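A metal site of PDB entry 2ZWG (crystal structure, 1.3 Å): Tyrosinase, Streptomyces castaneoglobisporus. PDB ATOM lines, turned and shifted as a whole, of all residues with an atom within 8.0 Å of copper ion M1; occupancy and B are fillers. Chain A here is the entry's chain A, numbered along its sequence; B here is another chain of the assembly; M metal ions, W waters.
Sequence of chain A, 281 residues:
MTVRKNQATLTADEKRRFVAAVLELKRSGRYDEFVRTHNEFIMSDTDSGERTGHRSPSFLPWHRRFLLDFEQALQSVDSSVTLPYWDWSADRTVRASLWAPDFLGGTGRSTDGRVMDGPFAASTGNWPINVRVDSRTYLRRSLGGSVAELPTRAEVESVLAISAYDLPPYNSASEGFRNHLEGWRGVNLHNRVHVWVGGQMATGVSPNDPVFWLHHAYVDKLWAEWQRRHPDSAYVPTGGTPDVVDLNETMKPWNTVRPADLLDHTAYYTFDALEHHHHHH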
ATOM      1  N   HIS A  38      -7.639  16.115   1.740  1.00  0.00           N
ATOM      2  CA  HIS A  38      -6.633  16.635   0.813  1.00  0.00           C
ATOM      3  C   HIS A  38      -6.496  15.769  -0.426  1.00  0.00           C
ATOM      4  O   HIS A  38      -6.406  16.275  -1.567  1.00  0.00           O
ATOM      5  CB  HIS A  38      -5.273  16.785   1.543  1.00  0.00           C
ATOM      6  CG  HIS A  38      -4.244  17.415   0.656  1.00  0.00           C
ATOM      7  ND1 HIS A  38      -3.359  16.665  -0.060  1.00  0.00           N
ATOM      8  CD2 HIS A  38      -3.972  18.711   0.348  1.00  0.00           C
ATOM      9  CE1 HIS A  38      -2.556  17.450  -0.785  1.00  0.00           C
ATOM     10  NE2 HIS A  38      -2.919  18.706  -0.548  1.00  0.00           N
ATOM     11  N   ILE A  42      -6.879  16.818  -4.345  1.00  0.00           N
ATOM     12  CA  ILE A  42      -5.810  16.872  -5.345  1.00  0.00           C
ATOM     13  C   ILE A  42      -6.101  15.900  -6.458  1.00  0.00           C
ATOM     14  O   ILE A  42      -5.627  16.029  -7.582  1.00  0.00           O
ATOM     15  CB  ILE A  42      -4.498  16.605  -4.586  1.00  0.00           C
ATOM     16  CG1 ILE A  42      -3.289  17.217  -5.324  1.00  0.00           C
ATOM     17  CG2 ILE A  42      -4.397  15.118  -4.317  1.00  0.00           C
ATOM     18  CD1 ILE A  42      -1.995  16.899  -4.611  1.00  0.00           C
ATOM     19  N   GLY A  53      -8.489  23.282  -4.697  1.00  0.00           N
ATOM     20  CA  GLY A  53      -7.445  23.302  -3.671  1.00  0.00           C
ATOM     21  C   GLY A  53      -6.062  23.468  -4.241  1.00  0.00           C
ATOM     22  O   GLY A  53      -5.176  23.837  -3.477  1.00  0.00           O
ATOM     23  N   HIS A  54      -5.870  23.169  -5.506  1.00  0.00           N
ATOM     24  CA  HIS A  54      -4.572  23.163  -6.174  1.00  0.00           C
ATOM     25  C   HIS A  54      -4.689  23.757  -7.558  1.00  0.00           C
ATOM     26  O   HIS A  54      -5.805  23.861  -8.120  1.00  0.00           O
ATOM     27  CB  HIS A  54      -3.974  21.735  -6.302  1.00  0.00           C
ATOM     28  CG  HIS A  54      -3.859  21.118  -4.927  1.00  0.00           C
ATOM     29  ND1 HIS A  54      -4.948  20.562  -4.280  1.00  0.00           N
ATOM     30  CD2 HIS A  54      -2.780  21.015  -4.127  1.00  0.00           C
ATOM     31  CE1 HIS A  54      -4.501  20.131  -3.090  1.00  0.00           C
ATOM     32  NE2 HIS A  54      -3.207  20.378  -2.971  1.00  0.00           N
ATOM     33  N   PHE A  59      -5.711  27.918  -4.467  1.00  0.00           N
ATOM     34  CA  PHE A  59      -4.685  27.157  -3.785  1.00  0.00           C
ATOM     35  C   PHE A  59      -4.304  27.763  -2.448  1.00  0.00           C
ATOM     36  O   PHE A  59      -4.239  27.077  -1.421  1.00  0.00           O
ATOM     37  CB  PHE A  59      -3.422  27.068  -4.666  1.00  0.00           C
ATOM     38  CG  PHE A  59      -2.189  26.483  -3.978  1.00  0.00           C
ATOM     39  CD1 PHE A  59      -2.068  25.172  -3.547  1.00  0.00           C
ATOM     40  CD2 PHE A  59      -1.108  27.344  -3.809  1.00  0.00           C
ATOM     41  CE1 PHE A  59      -0.905  24.699  -2.966  1.00  0.00           C
ATOM     42  CE2 PHE A  59       0.080  26.870  -3.238  1.00  0.00           C
ATOM     43  CZ  PHE A  59       0.175  25.554  -2.832  1.00  0.00           C
ATOM     44  N   HIS A  63      -5.709  26.227   1.198  1.00  0.00           N
ATOM     45  CA  HIS A  63      -4.795  25.668   2.198  1.00  0.00           C
ATOM     46  C   HIS A  63      -4.783  26.507   3.461  1.00  0.00           C
ATOM     47  O   HIS A  63      -4.603  25.960   4.546  1.00  0.00           O
ATOM     48  CB  HIS A  63      -3.385  25.500   1.603  1.00  0.00           C
ATOM     49  CG  HIS A  63      -3.282  24.304   0.731  1.00  0.00           C
ATOM     50  ND1 HIS A  63      -3.656  24.270  -0.615  1.00  0.00           N
ATOM     51  CD2 HIS A  63      -2.893  23.040   1.002  1.00  0.00           C
ATOM     52  CE1 HIS A  63      -3.476  23.063  -1.129  1.00  0.00           C
ATOM     53  NE2 HIS A  63      -3.005  22.284  -0.150  1.00  0.00           N
ATOM     54  N   GLU A 182       3.209  28.060  -5.908  1.00  0.00           N
ATOM     55  CA  GLU A 182       2.814  26.641  -5.944  1.00  0.00           C
ATOM     56  C   GLU A 182       3.882  25.782  -6.563  1.00  0.00           C
ATOM     57  O   GLU A 182       4.261  24.715  -6.040  1.00  0.00           O
ATOM     58  CB  GLU A 182       1.471  26.514  -6.686  1.00  0.00           C
ATOM     59  CG  GLU A 182       0.922  25.102  -6.598  1.00  0.00           C
ATOM     60  CD  GLU A 182      -0.502  24.994  -7.135  1.00  0.00           C
ATOM     61  OE1 GLU A 182      -1.072  25.993  -7.567  1.00  0.00           O
ATOM     62  OE2 GLU A 182      -1.018  23.850  -7.117  1.00  0.00           O
ATOM     63  N   HIS A 190       6.757  25.494  -3.686  1.00  0.00           N
ATOM     64  CA  HIS A 190       6.012  24.523  -2.872  1.00  0.00           C
ATOM     65  C   HIS A 190       6.026  23.099  -3.352  1.00  0.00           C
ATOM     66  O   HIS A 190       6.163  22.146  -2.564  1.00  0.00           O
ATOM     67  CB  HIS A 190       4.551  25.039  -2.768  1.00  0.00           C
ATOM     68  CG  HIS A 190       3.522  23.948  -2.616  1.00  0.00           C
ATOM     69  ND1 HIS A 190       2.988  23.284  -3.687  1.00  0.00           N
ATOM     70  CD2 HIS A 190       2.937  23.408  -1.519  1.00  0.00           C
ATOM     71  CE1 HIS A 190       2.100  22.352  -3.237  1.00  0.00           C
ATOM     72  NE2 HIS A 190       2.051  22.427  -1.903  1.00  0.00           N
ATOM     73  N   ASN A 191       5.929  22.884  -4.692  1.00  0.00           N
ATOM     74  CA  ASN A 191       5.946  21.518  -5.164  1.00  0.00           C
ATOM     75  C   ASN A 191       7.258  20.791  -4.890  1.00  0.00           C
ATOM     76  O   ASN A 191       7.285  19.618  -4.510  1.00  0.00           O
ATOM     77  CB  ASN A 191       5.712  21.500  -6.686  1.00  0.00           C
ATOM     78  CG  ASN A 191       4.253  21.689  -7.023  1.00  0.00           C
ATOM     79  OD1 ASN A 191       3.349  21.778  -6.186  1.00  0.00           O
ATOM     80  ND2 ASN A 191       3.956  21.753  -8.330  1.00  0.00           N
ATOM     81  N   VAL A 193       9.369  21.229  -2.515  1.00  0.00           N
ATOM     82  CA  VAL A 193       9.553  20.769  -1.114  1.00  0.00           C
ATOM     83  C   VAL A 193       8.847  19.433  -0.886  1.00  0.00           C
ATOM     84  O   VAL A 193       9.393  18.562  -0.198  1.00  0.00           O
ATOM     85  CB  VAL A 193       9.022  21.849  -0.188  1.00  0.00           C
ATOM     86  CG1 VAL A 193       9.154  21.358   1.271  1.00  0.00           C
ATOM     87  CG2 VAL A 193       9.769  23.166  -0.340  1.00  0.00           C
ATOM     88  N   HIS A 194       7.618  19.288  -1.437  1.00  0.00           N
ATOM     89  CA  HIS A 194       6.986  17.972  -1.321  1.00  0.00           C
ATOM     90  C   HIS A 194       7.846  16.873  -1.897  1.00  0.00           C
ATOM     91  O   HIS A 194       8.031  15.758  -1.362  1.00  0.00           O
ATOM     92  CB  HIS A 194       5.652  17.944  -2.075  1.00  0.00           C
ATOM     93  CG  HIS A 194       4.457  18.575  -1.404  1.00  0.00           C
ATOM     94  ND1 HIS A 194       3.715  17.857  -0.464  1.00  0.00           N
ATOM     95  CD2 HIS A 194       3.851  19.777  -1.537  1.00  0.00           C
ATOM     96  CE1 HIS A 194       2.710  18.633  -0.060  1.00  0.00           C
ATOM     97  NE2 HIS A 194       2.740  19.817  -0.683  1.00  0.00           N
ATOM     98  N   MET A 201       4.737  12.451   1.697  1.00  0.00           N
ATOM     99  CA  MET A 201       4.685  13.876   1.376  1.00  0.00           C
ATOM    100  C   MET A 201       4.817  14.146  -0.106  1.00  0.00           C
ATOM    101  O   MET A 201       4.415  15.245  -0.538  1.00  0.00           O
ATOM    102  CB  MET A 201       5.790  14.518   2.199  1.00  0.00           C
ATOM    103  CG  MET A 201       5.889  16.003   2.231  1.00  0.00           C
ATOM    104  SD  MET A 201       4.430  16.774   2.974  1.00  0.00           S
ATOM    105  CE  MET A 201       4.995  18.471   2.757  1.00  0.00           C
ATOM    106  N   THR A 203       3.001  12.537  -2.333  1.00  0.00           N
ATOM    107  CA  THR A 203       1.826  11.907  -2.872  1.00  0.00           C
ATOM    108  C   THR A 203       0.566  12.681  -2.506  1.00  0.00           C
ATOM    109  O   THR A 203       0.619  13.633  -1.713  1.00  0.00           O
ATOM    110  CB  THR A 203       1.606  10.452  -2.362  1.00  0.00           C
ATOM    111  OG1 THR A 203       1.161  10.509  -0.982  1.00  0.00           O
ATOM    112  CG2 THR A 203       2.895   9.661  -2.413  1.00  0.00           C
ATOM    113  N   SER A 206      -0.265  13.352   1.184  1.00  0.00           N
ATOM    114  CA  SER A 206       0.840  14.055   1.831  1.00  0.00           C
ATOM    115  C   SER A 206       0.532  14.506   3.241  1.00  0.00           C
ATOM    116  O   SER A 206       1.525  14.535   3.991  1.00  0.00           O
ATOM    117  CB  SER A 206       1.317  15.248   0.975  1.00  0.00           C
ATOM    118  OG  SER A 206       0.218  16.054   0.592  1.00  0.00           O
ATOM    119  N   PRO A 207      -0.662  14.841   3.686  1.00  0.00           N
ATOM    120  CA  PRO A 207      -0.808  15.143   5.127  1.00  0.00           C
ATOM    121  C   PRO A 207      -0.547  13.947   6.032  1.00  0.00           C
ATOM    122  O   PRO A 207      -0.535  14.146   7.262  1.00  0.00           O
ATOM    123  CB  PRO A 207      -2.265  15.601   5.273  1.00  0.00           C
ATOM    124  CG  PRO A 207      -2.596  16.077   3.869  1.00  0.00           C
ATOM    125  CD  PRO A 207      -1.940  15.061   2.987  1.00  0.00           C
ATOM    126  N   PHE A 212       3.731  18.118   6.591  1.00  0.00           N
ATOM    127  CA  PHE A 212       2.805  18.796   5.692  1.00  0.00           C
ATOM    128  C   PHE A 212       2.382  20.150   6.223  1.00  0.00           C
ATOM    129  O   PHE A 212       2.315  21.149   5.544  1.00  0.00           O
ATOM    130  CB  PHE A 212       1.571  17.871   5.503  1.00  0.00           C
ATOM    131  CG  PHE A 212       0.476  18.489   4.640  1.00  0.00           C
ATOM    132  CD1 PHE A 212      -0.556  19.280   5.176  1.00  0.00           C
ATOM    133  CD2 PHE A 212       0.503  18.253   3.265  1.00  0.00           C
ATOM    134  CE1 PHE A 212      -1.485  19.865   4.374  1.00  0.00           C
ATOM    135  CE2 PHE A 212      -0.453  18.854   2.489  1.00  0.00           C
ATOM    136  CZ  PHE A 212      -1.454  19.635   2.993  1.00  0.00           C
ATOM    137  N   HIS A 215       5.209  22.801   6.365  1.00  0.00           N
ATOM    138  CA  HIS A 215       5.489  23.267   5.004  1.00  0.00           C
ATOM    139  C   HIS A 215       4.383  24.241   4.630  1.00  0.00           C
ATOM    140  O   HIS A 215       4.656  25.383   4.228  1.00  0.00           O
ATOM    141  CB  HIS A 215       5.477  22.070   4.062  1.00  0.00           C
ATOM    142  CG  HIS A 215       5.583  22.414   2.614  1.00  0.00           C
ATOM    143  ND1 HIS A 215       6.354  23.522   2.240  1.00  0.00           N
ATOM    144  CD2 HIS A 215       5.030  21.842   1.521  1.00  0.00           C
ATOM    145  CE1 HIS A 215       6.250  23.578   0.897  1.00  0.00           C
ATOM    146  NE2 HIS A 215       5.485  22.600   0.435  1.00  0.00           N
ATOM    147  N   HIS A 216       3.099  23.847   4.723  1.00  0.00           N
ATOM    148  CA  HIS A 216       2.039  24.770   4.276  1.00  0.00           C
ATOM    149  C   HIS A 216       1.955  25.996   5.158  1.00  0.00           C
ATOM    150  O   HIS A 216       1.540  27.049   4.673  1.00  0.00           O
ATOM    151  CB  HIS A 216       0.655  24.038   4.123  1.00  0.00           C
ATOM    152  CG  HIS A 216       0.621  23.467   2.735  1.00  0.00           C
ATOM    153  ND1 HIS A 216       0.224  24.270   1.693  1.00  0.00           N
ATOM    154  CD2 HIS A 216       0.942  22.267   2.209  1.00  0.00           C
ATOM    155  CE1 HIS A 216       0.307  23.569   0.550  1.00  0.00           C
ATOM    156  NE2 HIS A 216       0.718  22.340   0.838  1.00  0.00           N
ATOM    157  N   VAL A 219       4.416  28.246   3.434  1.00  0.00           N
ATOM    158  CA  VAL A 219       3.815  28.705   2.156  1.00  0.00           C
ATOM    159  C   VAL A 219       2.840  29.807   2.447  1.00  0.00           C
ATOM    160  O   VAL A 219       2.760  30.823   1.759  1.00  0.00           O
ATOM    161  CB  VAL A 219       3.172  27.542   1.397  1.00  0.00           C
ATOM    162  CG1 VAL A 219       2.368  28.037   0.203  1.00  0.00           C
ATOM    163  CG2 VAL A 219       4.266  26.583   0.922  1.00  0.00           C
ATOM    164  N   DAH B  98       3.292  16.059  -7.160  1.00  0.00           N
ATOM    165  CA  DAH B  98       3.847  17.373  -7.257  1.00  0.00           C
ATOM    166  C   DAH B  98       5.061  17.417  -8.190  1.00  0.00           C
ATOM    167  O   DAH B  98       5.916  18.293  -8.096  1.00  0.00           O
ATOM    168  CB  DAH B  98       4.295  17.840  -5.844  1.00  0.00           C
ATOM    169  CG  DAH B  98       3.201  17.687  -4.798  1.00  0.00           C
ATOM    170  CD1 DAH B  98       3.094  16.540  -4.013  1.00  0.00           C
ATOM    171  CD2 DAH B  98       2.295  18.734  -4.599  1.00  0.00           C
ATOM    172  CE1 DAH B  98       2.114  16.395  -3.062  1.00  0.00           C
ATOM    173  CE2 DAH B  98       1.306  18.595  -3.648  1.00  0.00           C
ATOM    174  CZ  DAH B  98       1.224  17.443  -2.896  1.00  0.00           C
ATOM    175  OE2 DAH B  98       0.360  19.478  -3.336  1.00  0.00           O
ATOM    176  OH  DAH B  98       0.231  17.385  -1.952  1.00  0.00           O
HETATM  177 CU    CU M   1       1.124  21.086  -0.868  1.00  0.00          CU
HETATM  178 CU    CU M   2      -1.982  20.308  -1.335  1.00  0.00          CU
HETATM  179  O   HOH W   1      -0.709  21.511  -2.148  1.00  0.00           O
HETATM  180  O   HOH W   2      -0.316  19.785  -0.518  1.00  0.00           O
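A ring nitrogen (ND1) of His 190 is in hydrogen-bond range of the side-chain amide oxygen of Asn 191 (2.9 Å). The backbone carbonyl oxygen of His 190 lies within hydrogen-bond range of a ring nitrogen (NE2) of His 215, at 3.1 Å. O of Glu 182 sits at hydrogen-bond distance from ND1 of His 190 (3.0 Å). The backbone carbonyl oxygen of Met 201 lies within hydrogen-bond range of a ring nitrogen (ND1) of His 194, at 2.7 Å. OH of DAH 98 of chain B sits at hydrogen-bond distance from the side-chain hydroxyl of Ser 206 (2.9 Å).
A ring nitrogen (NE2) of His 190 is bound to copper ion M1 (1.9 Å). Copper ion M1 is bound by water W2 (2.0 Å). Copper ion M1 is bound by NE2 of His 194, 2.1 Å away. Copper ion M1 is bound by NE2 of His 216 (2.2 Å). Copper ion M1 is bound by water W1, 2.3 Å away.
Residues that only touch copper ion M1: DAH 98 of chain B (3.0 Å). Of the 20 residues printed, 4 come within 4 Å of copper ion M1.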
